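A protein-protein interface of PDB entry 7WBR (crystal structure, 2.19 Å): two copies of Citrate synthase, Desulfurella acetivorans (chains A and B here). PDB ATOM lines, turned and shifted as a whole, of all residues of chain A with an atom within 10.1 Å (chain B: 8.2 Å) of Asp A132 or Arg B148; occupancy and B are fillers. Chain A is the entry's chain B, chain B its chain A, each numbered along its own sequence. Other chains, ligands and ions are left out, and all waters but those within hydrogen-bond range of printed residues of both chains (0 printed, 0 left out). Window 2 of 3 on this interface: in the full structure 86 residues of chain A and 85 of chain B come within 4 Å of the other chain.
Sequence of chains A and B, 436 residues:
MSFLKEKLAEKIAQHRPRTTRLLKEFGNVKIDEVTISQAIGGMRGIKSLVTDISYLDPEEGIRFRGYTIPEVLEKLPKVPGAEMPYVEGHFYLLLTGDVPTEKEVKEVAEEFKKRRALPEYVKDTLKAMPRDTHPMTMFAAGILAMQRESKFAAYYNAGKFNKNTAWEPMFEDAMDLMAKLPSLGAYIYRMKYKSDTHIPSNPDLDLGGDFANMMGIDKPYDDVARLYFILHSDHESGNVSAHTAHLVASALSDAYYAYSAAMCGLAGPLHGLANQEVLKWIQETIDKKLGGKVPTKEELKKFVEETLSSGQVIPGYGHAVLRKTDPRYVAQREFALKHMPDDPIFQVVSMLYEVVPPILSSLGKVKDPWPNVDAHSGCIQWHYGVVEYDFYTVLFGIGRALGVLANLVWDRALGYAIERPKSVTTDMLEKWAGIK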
ATOM      1  N   LEU A 126      11.248  33.708  -4.434  1.00  0.00           N
ATOM      2  CA  LEU A 126      11.487  32.352  -3.897  1.00  0.00           C
ATOM      3  C   LEU A 126      11.077  31.254  -4.831  1.00  0.00           C
ATOM      4  O   LEU A 126      11.614  30.154  -4.704  1.00  0.00           O
ATOM      5  CB  LEU A 126      10.835  32.106  -2.520  1.00  0.00           C
ATOM      6  CG  LEU A 126      11.223  33.091  -1.415  1.00  0.00           C
ATOM      7  CD1 LEU A 126      10.466  32.928  -0.104  1.00  0.00           C
ATOM      8  CD2 LEU A 126      12.668  33.047  -1.121  1.00  0.00           C
ATOM      9  N   LYS A 127      10.134  31.507  -5.748  1.00  0.00           N
ATOM     10  CA  LYS A 127       9.821  30.522  -6.786  1.00  0.00           C
ATOM     11  C   LYS A 127      10.838  30.569  -7.932  1.00  0.00           C
ATOM     12  O   LYS A 127      11.009  29.598  -8.615  1.00  0.00           O
ATOM     13  CB  LYS A 127       8.441  30.761  -7.435  1.00  0.00           C
ATOM     14  CG  LYS A 127       7.228  30.686  -6.498  1.00  0.00           C
ATOM     15  CD  LYS A 127       6.037  31.229  -7.275  1.00  0.00           C
ATOM     16  CE  LYS A 127       4.780  31.324  -6.478  1.00  0.00           C
ATOM     17  NZ  LYS A 127       3.625  31.538  -7.431  1.00  0.00           N
ATOM     18  N   ALA A 128      11.473  31.699  -8.190  1.00  0.00           N
ATOM     19  CA  ALA A 128      12.485  31.739  -9.229  1.00  0.00           C
ATOM     20  C   ALA A 128      13.698  31.048  -8.737  1.00  0.00           C
ATOM     21  O   ALA A 128      14.354  30.373  -9.507  1.00  0.00           O
ATOM     22  CB  ALA A 128      12.807  33.165  -9.666  1.00  0.00           C
ATOM     23  N   MET A 129      13.980  31.150  -7.441  1.00  0.00           N
ATOM     24  CA  MET A 129      15.041  30.358  -6.844  1.00  0.00           C
ATOM     25  C   MET A 129      14.729  28.866  -6.973  1.00  0.00           C
ATOM     26  O   MET A 129      13.576  28.450  -6.779  1.00  0.00           O
ATOM     27  CB  MET A 129      15.232  30.737  -5.402  1.00  0.00           C
ATOM     28  CG  MET A 129      15.817  32.136  -5.263  1.00  0.00           C
ATOM     29  SD  MET A 129      15.900  32.660  -3.553  1.00  0.00           S
ATOM     30  CE  MET A 129      17.478  31.916  -3.133  1.00  0.00           C
ATOM     31  N   PRO A 130      15.748  28.054  -7.285  1.00  0.00           N
ATOM     32  CA  PRO A 130      15.411  26.622  -7.488  1.00  0.00           C
ATOM     33  C   PRO A 130      14.789  26.000  -6.248  1.00  0.00           C
ATOM     34  O   PRO A 130      15.238  26.283  -5.118  1.00  0.00           O
ATOM     35  CB  PRO A 130      16.783  26.016  -7.790  1.00  0.00           C
ATOM     36  CG  PRO A 130      17.427  27.121  -8.630  1.00  0.00           C
ATOM     37  CD  PRO A 130      17.034  28.396  -7.924  1.00  0.00           C
ATOM     38  N   ARG A 131      13.736  25.220  -6.423  1.00  0.00           N
ATOM     39  CA  ARG A 131      13.015  24.706  -5.282  1.00  0.00           C
ATOM     40  C   ARG A 131      13.888  23.863  -4.371  1.00  0.00           C
ATOM     41  O   ARG A 131      13.560  23.742  -3.186  1.00  0.00           O
ATOM     42  CB  ARG A 131      11.746  23.933  -5.696  1.00  0.00           C
ATOM     43  CG  ARG A 131      10.827  23.504  -4.529  1.00  0.00           C
ATOM     44  CD  ARG A 131      10.171  24.713  -3.806  1.00  0.00           C
ATOM     45  NE  ARG A 131       9.564  25.632  -4.779  1.00  0.00           N
ATOM     46  CZ  ARG A 131       8.277  25.708  -5.088  1.00  0.00           C
ATOM     47  NH1 ARG A 131       7.337  25.041  -4.424  1.00  0.00           N
ATOM     48  NH2 ARG A 131       7.912  26.529  -6.005  1.00  0.00           N
ATOM     49  N   ASP A 132      15.004  23.309  -4.888  1.00  0.00           N
ATOM     50  CA  ASP A 132      15.895  22.488  -4.044  1.00  0.00           C
ATOM     51  C   ASP A 132      16.854  23.358  -3.228  1.00  0.00           C
ATOM     52  O   ASP A 132      17.704  22.861  -2.527  1.00  0.00           O
ATOM     53  CB  ASP A 132      16.637  21.427  -4.853  1.00  0.00           C
ATOM     54  CG  ASP A 132      17.390  22.010  -6.064  1.00  0.00           C
ATOM     55  OD1 ASP A 132      17.365  23.217  -6.310  1.00  0.00           O
ATOM     56  OD2 ASP A 132      17.990  21.252  -6.789  1.00  0.00           O
ATOM     57  N   THR A 133      16.722  24.671  -3.339  1.00  0.00           N
ATOM     58  CA  THR A 133      17.448  25.567  -2.474  1.00  0.00           C
ATOM     59  C   THR A 133      17.115  25.362  -1.002  1.00  0.00           C
ATOM     60  O   THR A 133      15.951  25.158  -0.606  1.00  0.00           O
ATOM     61  CB  THR A 133      17.169  27.034  -2.871  1.00  0.00           C
ATOM     62  OG1 THR A 133      17.308  27.167  -4.273  1.00  0.00           O
ATOM     63  CG2 THR A 133      18.094  27.952  -2.237  1.00  0.00           C
ATOM     64  N   HIS A 134      18.165  25.439  -0.207  1.00  0.00           N
ATOM     65  CA  HIS A 134      18.117  25.220   1.205  1.00  0.00           C
ATOM     66  C   HIS A 134      17.216  26.323   1.799  1.00  0.00           C
ATOM     67  O   HIS A 134      17.228  27.484   1.333  1.00  0.00           O
ATOM     68  CB  HIS A 134      19.553  25.346   1.738  1.00  0.00           C
ATOM     69  CG  HIS A 134      19.710  24.979   3.151  1.00  0.00           C
ATOM     70  ND1 HIS A 134      19.388  25.843   4.168  1.00  0.00           N
ATOM     71  CD2 HIS A 134      20.195  23.874   3.734  1.00  0.00           C
ATOM     72  CE1 HIS A 134      19.623  25.276   5.329  1.00  0.00           C
ATOM     73  NE2 HIS A 134      20.152  24.094   5.091  1.00  0.00           N
ATOM     74  N   PRO A 135      16.439  25.982   2.822  1.00  0.00           N
ATOM     75  CA  PRO A 135      15.408  26.971   3.261  1.00  0.00           C
ATOM     76  C   PRO A 135      16.023  28.204   3.915  1.00  0.00           C
ATOM     77  O   PRO A 135      15.458  29.267   3.897  1.00  0.00           O
ATOM     78  CB  PRO A 135      14.575  26.171   4.281  1.00  0.00           C
ATOM     79  CG  PRO A 135      15.454  25.075   4.741  1.00  0.00           C
ATOM     80  CD  PRO A 135      16.295  24.686   3.534  1.00  0.00           C
ATOM     81  N   MET A 136      17.175  28.055   4.520  1.00  0.00           N
ATOM     82  CA  MET A 136      17.944  29.225   4.972  1.00  0.00           C
ATOM     83  C   MET A 136      18.403  30.176   3.885  1.00  0.00           C
ATOM     84  O   MET A 136      18.465  31.383   4.121  1.00  0.00           O
ATOM     85  CB  MET A 136      19.156  28.849   5.854  1.00  0.00           C
ATOM     86  CG  MET A 136      18.774  28.508   7.270  1.00  0.00           C
ATOM     87  SD  MET A 136      18.027  29.840   8.233  1.00  0.00           S
ATOM     88  CE  MET A 136      19.348  30.932   8.661  1.00  0.00           C
ATOM     89  N   THR A 137      18.774  29.643   2.736  1.00  0.00           N
ATOM     90  CA  THR A 137      19.149  30.505   1.627  1.00  0.00           C
ATOM     91  C   THR A 137      17.889  31.264   1.126  1.00  0.00           C
ATOM     92  O   THR A 137      17.924  32.456   0.953  1.00  0.00           O
ATOM     93  CB  THR A 137      19.818  29.704   0.523  1.00  0.00           C
ATOM     94  OG1 THR A 137      20.959  29.041   1.077  1.00  0.00           O
ATOM     95  CG2 THR A 137      20.237  30.612  -0.600  1.00  0.00           C
ATOM     96  N   MET A 138      16.769  30.557   0.977  1.00  0.00           N
ATOM     97  CA  MET A 138      15.481  31.208   0.700  1.00  0.00           C
ATOM     98  C   MET A 138      15.151  32.286   1.713  1.00  0.00           C
ATOM     99  O   MET A 138      14.665  33.305   1.326  1.00  0.00           O
ATOM    100  CB  MET A 138      14.334  30.224   0.632  1.00  0.00           C
ATOM    101  CG  MET A 138      14.414  29.327  -0.580  1.00  0.00           C
ATOM    102  SD  MET A 138      12.913  28.351  -0.715  1.00  0.00           S
ATOM    103  CE  MET A 138      13.223  27.503  -2.259  1.00  0.00           C
ATOM    104  N   ILE A 188       8.022  29.635   3.173  1.00  0.00           N
ATOM    105  CA  ILE A 188       9.103  28.654   2.849  1.00  0.00           C
ATOM    106  C   ILE A 188       8.750  27.225   3.254  1.00  0.00           C
ATOM    107  O   ILE A 188       8.943  26.280   2.456  1.00  0.00           O
ATOM    108  CB  ILE A 188      10.476  29.086   3.417  1.00  0.00           C
ATOM    109  CG1 ILE A 188      11.029  30.285   2.567  1.00  0.00           C
ATOM    110  CG2 ILE A 188      11.526  28.028   3.191  1.00  0.00           C
ATOM    111  CD1 ILE A 188      11.845  31.289   3.326  1.00  0.00           C
ATOM    112  N   MET A 191       5.967  25.952   0.854  1.00  0.00           N
ATOM    113  CA  MET A 191       6.368  25.779  -0.545  1.00  0.00           C
ATOM    114  C   MET A 191       7.341  24.660  -0.799  1.00  0.00           C
ATOM    115  O   MET A 191       7.245  24.022  -1.826  1.00  0.00           O
ATOM    116  CB  MET A 191       6.826  27.083  -1.208  1.00  0.00           C
ATOM    117  CG  MET A 191       8.037  27.744  -0.603  1.00  0.00           C
ATOM    118  SD  MET A 191       9.389  27.623  -1.747  1.00  0.00           S
ATOM    119  CE  MET A 191       8.815  28.691  -3.069  1.00  0.00           C
ATOM    120  N   LYS A 192       8.175  24.351   0.178  1.00  0.00           N
ATOM    121  CA  LYS A 192       9.195  23.365   0.054  1.00  0.00           C
ATOM    122  C   LYS A 192       8.691  21.992   0.540  1.00  0.00           C
ATOM    123  O   LYS A 192       8.926  20.994  -0.130  1.00  0.00           O
ATOM    124  CB  LYS A 192      10.462  23.775   0.877  1.00  0.00           C
ATOM    125  CG  LYS A 192      11.588  24.378   0.071  1.00  0.00           C
ATOM    126  CD  LYS A 192      12.895  24.351   0.846  1.00  0.00           C
ATOM    127  CE  LYS A 192      13.734  23.155   0.525  1.00  0.00           C
ATOM    128  NZ  LYS A 192      14.365  23.215  -0.816  1.00  0.00           N
ATOM    129  N   TYR A 193       7.992  21.933   1.661  1.00  0.00           N
ATOM    130  CA  TYR A 193       7.779  20.635   2.353  1.00  0.00           C
ATOM    131  C   TYR A 193       6.354  20.222   2.536  1.00  0.00           C
ATOM    132  O   TYR A 193       6.145  19.128   2.926  1.00  0.00           O
ATOM    133  CB  TYR A 193       8.408  20.652   3.737  1.00  0.00           C
ATOM    134  CG  TYR A 193       9.854  21.096   3.786  1.00  0.00           C
ATOM    135  CD1 TYR A 193      10.870  20.341   3.133  1.00  0.00           C
ATOM    136  CD2 TYR A 193      10.220  22.272   4.459  1.00  0.00           C
ATOM    137  CE1 TYR A 193      12.187  20.752   3.198  1.00  0.00           C
ATOM    138  CE2 TYR A 193      11.550  22.667   4.557  1.00  0.00           C
ATOM    139  CZ  TYR A 193      12.520  21.922   3.931  1.00  0.00           C
ATOM    140  OH  TYR A 193      13.807  22.372   3.988  1.00  0.00           O
ATOM    141  N   ASP A 390      16.375  20.748   8.044  1.00  0.00           N
ATOM    142  CA  ASP A 390      16.961  21.987   7.532  1.00  0.00           C
ATOM    143  C   ASP A 390      16.144  23.215   7.942  1.00  0.00           C
ATOM    144  O   ASP A 390      16.711  24.281   8.205  1.00  0.00           O
ATOM    145  CB  ASP A 390      17.113  21.946   6.013  1.00  0.00           C
ATOM    146  CG  ASP A 390      18.134  20.926   5.530  1.00  0.00           C
ATOM    147  OD1 ASP A 390      19.034  20.463   6.246  1.00  0.00           O
ATOM    148  OD2 ASP A 390      18.017  20.579   4.376  1.00  0.00           O
ATOM    149  N   PRO B 119      24.546  30.744 -13.956  1.00  0.00           N
ATOM    150  CA  PRO B 119      23.315  29.930 -13.956  1.00  0.00           C
ATOM    151  C   PRO B 119      22.095  30.727 -14.424  1.00  0.00           C
ATOM    152  O   PRO B 119      21.936  31.907 -14.077  1.00  0.00           O
ATOM    153  CB  PRO B 119      23.170  29.542 -12.507  1.00  0.00           C
ATOM    154  CG  PRO B 119      24.600  29.490 -12.002  1.00  0.00           C
ATOM    155  CD  PRO B 119      25.224  30.686 -12.656  1.00  0.00           C
ATOM    156  N   TYR B 121      19.043  30.371 -13.469  1.00  0.00           N
ATOM    157  CA  TYR B 121      18.166  30.723 -12.319  1.00  0.00           C
ATOM    158  C   TYR B 121      18.661  31.951 -11.601  1.00  0.00           C
ATOM    159  O   TYR B 121      17.950  32.557 -10.797  1.00  0.00           O
ATOM    160  CB  TYR B 121      18.009  29.550 -11.341  1.00  0.00           C
ATOM    161  CG  TYR B 121      19.279  29.219 -10.515  1.00  0.00           C
ATOM    162  CD1 TYR B 121      19.687  30.000  -9.449  1.00  0.00           C
ATOM    163  CD2 TYR B 121      20.036  28.085 -10.820  1.00  0.00           C
ATOM    164  CE1 TYR B 121      20.851  29.682  -8.718  1.00  0.00           C
ATOM    165  CE2 TYR B 121      21.166  27.753 -10.123  1.00  0.00           C
ATOM    166  CZ  TYR B 121      21.584  28.556  -9.070  1.00  0.00           C
ATOM    167  OH  TYR B 121      22.715  28.177  -8.398  1.00  0.00           O
ATOM    168  N   GLY B 142      22.071  37.659  -6.023  1.00  0.00           N
ATOM    169  CA  GLY B 142      22.645  36.793  -7.066  1.00  0.00           C
ATOM    170  C   GLY B 142      23.714  35.823  -6.541  1.00  0.00           C
ATOM    171  O   GLY B 142      23.698  34.621  -6.864  1.00  0.00           O
ATOM    172  N   ILE B 143      24.648  36.377  -5.750  1.00  0.00           N
ATOM    173  CA  ILE B 143      25.648  35.588  -5.038  1.00  0.00           C
ATOM    174  C   ILE B 143      24.964  34.600  -4.085  1.00  0.00           C
ATOM    175  O   ILE B 143      25.254  33.447  -4.116  1.00  0.00           O
ATOM    176  CB  ILE B 143      26.623  36.480  -4.212  1.00  0.00           C
ATOM    177  CG1 ILE B 143      27.313  37.519  -5.078  1.00  0.00           C
ATOM    178  CG2 ILE B 143      27.673  35.612  -3.489  1.00  0.00           C
ATOM    179  CD1 ILE B 143      27.732  38.721  -4.288  1.00  0.00           C
ATOM    180  N   LEU B 144      24.023  35.079  -3.264  1.00  0.00           N
ATOM    181  CA  LEU B 144      23.280  34.234  -2.338  1.00  0.00           C
ATOM    182  C   LEU B 144      22.543  33.060  -3.038  1.00  0.00           C
ATOM    183  O   LEU B 144      22.620  31.923  -2.582  1.00  0.00           O
ATOM    184  CB  LEU B 144      22.336  35.062  -1.532  1.00  0.00           C
ATOM    185  CG  LEU B 144      21.451  34.306  -0.580  1.00  0.00           C
ATOM    186  CD1 LEU B 144      22.242  33.576   0.491  1.00  0.00           C
ATOM    187  CD2 LEU B 144      20.453  35.269   0.045  1.00  0.00           C
ATOM    188  N   ALA B 145      21.861  33.300  -4.146  1.00  0.00           N
ATOM    189  CA  ALA B 145      21.148  32.194  -4.849  1.00  0.00           C
ATOM    190  C   ALA B 145      22.091  31.097  -5.318  1.00  0.00           C
ATOM    191  O   ALA B 145      21.731  29.928  -5.269  1.00  0.00           O
ATOM    192  CB  ALA B 145      20.401  32.729  -6.027  1.00  0.00           C
ATOM    193  N   MET B 146      23.330  31.472  -5.705  1.00  0.00           N
ATOM    194  CA  MET B 146      24.309  30.475  -6.111  1.00  0.00           C
ATOM    195  C   MET B 146      24.860  29.622  -4.986  1.00  0.00           C
ATOM    196  O   MET B 146      25.628  28.705  -5.268  1.00  0.00           O
ATOM    197  CB  MET B 146      25.460  31.148  -6.883  1.00  0.00           C
ATOM    198  CG  MET B 146      24.971  31.714  -8.242  1.00  0.00           C
ATOM    199  SD  MET B 146      26.329  32.124  -9.347  1.00  0.00           S
ATOM    200  CE  MET B 146      26.846  33.537  -8.448  1.00  0.00           C
ATOM    201  N   GLN B 147      24.456  29.879  -3.735  1.00  0.00           N
ATOM    202  CA  GLN B 147      24.758  28.997  -2.620  1.00  0.00           C
ATOM    203  C   GLN B 147      24.344  27.539  -2.872  1.00  0.00           C
ATOM    204  O   GLN B 147      25.015  26.604  -2.425  1.00  0.00           O
ATOM    205  CB  GLN B 147      24.091  29.514  -1.330  1.00  0.00           C
ATOM    206  CG  GLN B 147      24.593  28.835  -0.064  1.00  0.00           C
ATOM    207  CD  GLN B 147      23.870  27.529   0.299  1.00  0.00           C
ATOM    208  OE1 GLN B 147      22.700  27.350   0.029  1.00  0.00           O
ATOM    209  NE2 GLN B 147      24.577  26.650   1.003  1.00  0.00           N
ATOM    210  N   ARG B 148      23.250  27.355  -3.603  1.00  0.00           N
ATOM    211  CA  ARG B 148      22.822  26.027  -4.091  1.00  0.00           C
ATOM    212  C   ARG B 148      23.993  25.233  -4.677  1.00  0.00           C
ATOM    213  O   ARG B 148      23.974  24.037  -4.603  1.00  0.00           O
ATOM    214  CB  ARG B 148      21.713  26.208  -5.171  1.00  0.00           C
ATOM    215  CG  ARG B 148      21.432  25.025  -6.091  1.00  0.00           C
ATOM    216  CD  ARG B 148      20.361  25.389  -7.114  1.00  0.00           C
ATOM    217  NE  ARG B 148      19.734  24.179  -7.580  1.00  0.00           N
ATOM    218  CZ  ARG B 148      20.217  23.396  -8.529  1.00  0.00           C
ATOM    219  NH1 ARG B 148      21.343  23.702  -9.180  1.00  0.00           N
ATOM    220  NH2 ARG B 148      19.568  22.295  -8.839  1.00  0.00           N
ATOM    221  N   GLU B 149      24.964  25.907  -5.312  1.00  0.00           N
ATOM    222  CA  GLU B 149      26.117  25.211  -5.962  1.00  0.00           C
ATOM    223  C   GLU B 149      27.319  24.942  -5.017  1.00  0.00           C
ATOM    224  O   GLU B 149      28.314  24.375  -5.437  1.00  0.00           O
ATOM    225  CB  GLU B 149      26.600  25.989  -7.177  1.00  0.00           C
ATOM    226  CG  GLU B 149      25.476  26.521  -8.096  1.00  0.00           C
ATOM    227  CD  GLU B 149      24.462  25.453  -8.514  1.00  0.00           C
ATOM    228  OE1 GLU B 149      24.820  24.263  -8.611  1.00  0.00           O
ATOM    229  OE2 GLU B 149      23.296  25.817  -8.728  1.00  0.00           O
ATOM    230  N   SER B 150      27.242  25.352  -3.756  1.00  0.00           N
ATOM    231  CA  SER B 150      28.429  25.318  -2.886  1.00  0.00           C
ATOM    232  C   SER B 150      28.999  23.917  -2.717  1.00  0.00           C
ATOM    233  O   SER B 150      28.320  23.055  -2.151  1.00  0.00           O
ATOM    234  CB  SER B 150      28.122  25.847  -1.502  1.00  0.00           C
ATOM    235  OG  SER B 150      29.303  25.813  -0.765  1.00  0.00           O
ATOM    236  N   LYS B 151      30.224  23.710  -3.215  1.00  0.00           N
ATOM    237  CA  LYS B 151      30.960  22.503  -2.916  1.00  0.00           C
ATOM    238  C   LYS B 151      31.288  22.388  -1.433  1.00  0.00           C
ATOM    239  O   LYS B 151      31.253  21.282  -0.895  1.00  0.00           O
ATOM    240  CB  LYS B 151      32.237  22.453  -3.769  1.00  0.00           C
ATOM    241  CG  LYS B 151      31.890  22.093  -5.225  1.00  0.00           C
ATOM    242  CD  LYS B 151      32.617  22.948  -6.232  1.00  0.00           C
ATOM    243  CE  LYS B 151      31.987  22.804  -7.619  1.00  0.00           C
ATOM    244  NZ  LYS B 151      32.885  23.385  -8.654  1.00  0.00           N
ATOM    245  N   ALA B 153      29.536  23.611   1.173  1.00  0.00           N
ATOM    246  CA  ALA B 153      28.298  23.145   1.809  1.00  0.00           C
ATOM    247  C   ALA B 153      27.997  21.670   1.522  1.00  0.00           C
ATOM    248  O   ALA B 153      27.644  20.917   2.429  1.00  0.00           O
ATOM    249  CB  ALA B 153      27.129  24.020   1.403  1.00  0.00           C
ATOM    250  N   ALA B 154      28.169  21.228   0.277  1.00  0.00           N
ATOM    251  CA  ALA B 154      27.914  19.808  -0.027  1.00  0.00           C
ATOM    252  C   ALA B 154      28.906  18.829   0.745  1.00  0.00           C
ATOM    253  O   ALA B 154      28.520  17.777   1.314  1.00  0.00           O
ATOM    254  CB  ALA B 154      27.970  19.583  -1.532  1.00  0.00           C
ATOM    255  N   ASP B 173      34.983  26.698  -4.439  1.00  0.00           N
ATOM    256  CA  ASP B 173      33.926  27.681  -4.436  1.00  0.00           C
ATOM    257  C   ASP B 173      34.451  29.065  -4.796  1.00  0.00           C
ATOM    258  O   ASP B 173      33.776  29.822  -5.525  1.00  0.00           O
ATOM    259  CB  ASP B 173      33.175  27.753  -3.077  1.00  0.00           C
ATOM    260  CG  ASP B 173      32.179  26.587  -2.857  1.00  0.00           C
ATOM    261  OD1 ASP B 173      31.799  25.874  -3.832  1.00  0.00           O
ATOM    262  OD2 ASP B 173      31.728  26.396  -1.684  1.00  0.00           O
ATOM    263  N   ASP B 254      29.501  28.666   3.891  1.00  0.00           N
ATOM    264  CA  ASP B 254      30.230  28.746   2.618  1.00  0.00           C
ATOM    265  C   ASP B 254      30.466  30.180   2.077  1.00  0.00           C
ATOM    266  O   ASP B 254      29.895  31.149   2.583  1.00  0.00           O
ATOM    267  CB  ASP B 254      29.585  27.800   1.602  1.00  0.00           C
ATOM    268  CG  ASP B 254      28.207  28.252   1.150  1.00  0.00           C
ATOM    269  OD1 ASP B 254      28.144  29.197   0.357  1.00  0.00           O
ATOM    270  OD2 ASP B 254      27.197  27.626   1.555  1.00  0.00           O
ATOM    271  N   TYR B 256      29.457  31.555  -0.510  1.00  0.00           N
ATOM    272  CA  TYR B 256      28.301  32.240  -1.118  1.00  0.00           C
ATOM    273  C   TYR B 256      27.529  32.986  -0.035  1.00  0.00           C
ATOM    274  O   TYR B 256      27.281  34.186  -0.151  1.00  0.00           O
ATOM    275  CB  TYR B 256      27.402  31.325  -1.939  1.00  0.00           C
ATOM    276  CG  TYR B 256      28.069  30.746  -3.153  1.00  0.00           C
ATOM    277  CD1 TYR B 256      28.032  31.389  -4.370  1.00  0.00           C
ATOM    278  CD2 TYR B 256      28.757  29.542  -3.077  1.00  0.00           C
ATOM    279  CE1 TYR B 256      28.633  30.838  -5.499  1.00  0.00           C
ATOM    280  CE2 TYR B 256      29.383  28.988  -4.190  1.00  0.00           C
ATOM    281  CZ  TYR B 256      29.303  29.635  -5.424  1.00  0.00           C
ATOM    282  OH  TYR B 256      29.926  29.061  -6.535  1.00  0.00           O
ATOM    283  N   TYR B 257      27.258  32.300   1.066  1.00  0.00           N
ATOM    284  CA  TYR B 257      26.713  32.973   2.227  1.00  0.00           C
ATOM    285  C   TYR B 257      27.597  34.149   2.678  1.00  0.00           C
ATOM    286  O   TYR B 257      27.115  35.240   2.948  1.00  0.00           O
ATOM    287  CB  TYR B 257      26.604  31.979   3.380  1.00  0.00           C
ATOM    288  CG  TYR B 257      25.426  31.066   3.360  1.00  0.00           C
ATOM    289  CD1 TYR B 257      24.145  31.552   3.158  1.00  0.00           C
ATOM    290  CD2 TYR B 257      25.576  29.726   3.605  1.00  0.00           C
ATOM    291  CE1 TYR B 257      23.053  30.730   3.126  1.00  0.00           C
ATOM    292  CE2 TYR B 257      24.484  28.874   3.603  1.00  0.00           C
ATOM    293  CZ  TYR B 257      23.219  29.381   3.336  1.00  0.00           C
ATOM    294  OH  TYR B 257      22.090  28.542   3.331  1.00  0.00           O
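The side-chain hydroxyl (OH) of Tyr B121 is in hydrogen-bond range of the side-chain carboxylate (OE2) of Glu B149, at 2.5 Å.
OD2 of Asp B254 is in hydrogen-bond range of NE2 of Gln B147.
The guanidinium group (NH1) of Arg B148 is in salt-bridge range of the side-chain carboxylate (OE2) of Glu B149 (2.9 Å).
The side-chain carboxylate (OD1) of Asp B254 sits at hydrogen-bond distance from the backbone NH (N) of Tyr B257, 3.3 Å away.
The side-chain hydroxyl of Thr A133 lies within hydrogen-bond range of the backbone carbonyl oxygen of Pro A130 (2.4 Å).
ND1 of His A134 lies within hydrogen-bond range of N of Met A136, at 3.1 Å.
The side-chain hydroxyl (OG1) of Thr A137 lies within hydrogen-bond range of the side-chain amide oxygen (OE1) of Gln B147.
NH2 of Arg B148 lies within salt-bridge range of OD2 of Asp A132.
The side-chain hydroxyl of Tyr B257 lies within hydrogen-bond range of the side-chain hydroxyl of Thr A137, 2.6 Å away.
No position is printed for both chains.
Asp A132 touches one residue of chain B.
Of the printed residues of chain A, Tyr B121 touches Pro A130 (3.4 Å).
Gln B147 touches just one residue of chain A: Thr A137 (2.6 Å).
Printed residues of chain A within 4 Å of Arg B148: Pro A130 and Asp A132.
No residue of chain A comes within 4 Å of Glu B149.
Of the printed residues of chain A, Tyr B257 touches His A134, Met A136 and Thr A137.
Of the 18 printed residues of chain A, 5 touch a printed residue of chain B.
Along chain B the printed residues that touch a printed residue of chain A span positions 121 to 257.
Among the printed residues, 8 pairs touch across the chains.
Among the printed residues, Asp or Glu carboxylates within 4 Å of a Lys or Arg side-chain nitrogen of the other chain: Asp A132 with Arg B148.
Among the printed residues, pairs that only touch across the chains: Thr A137 with Leu B144 (3.4 Å), Pro A130 with Tyr B121 (3.4 Å), Pro A130 with Arg B148 (3.5 Å), Met A136 with Tyr B257 (3.9 Å) and His A134 with Tyr B257 (3.9 Å).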
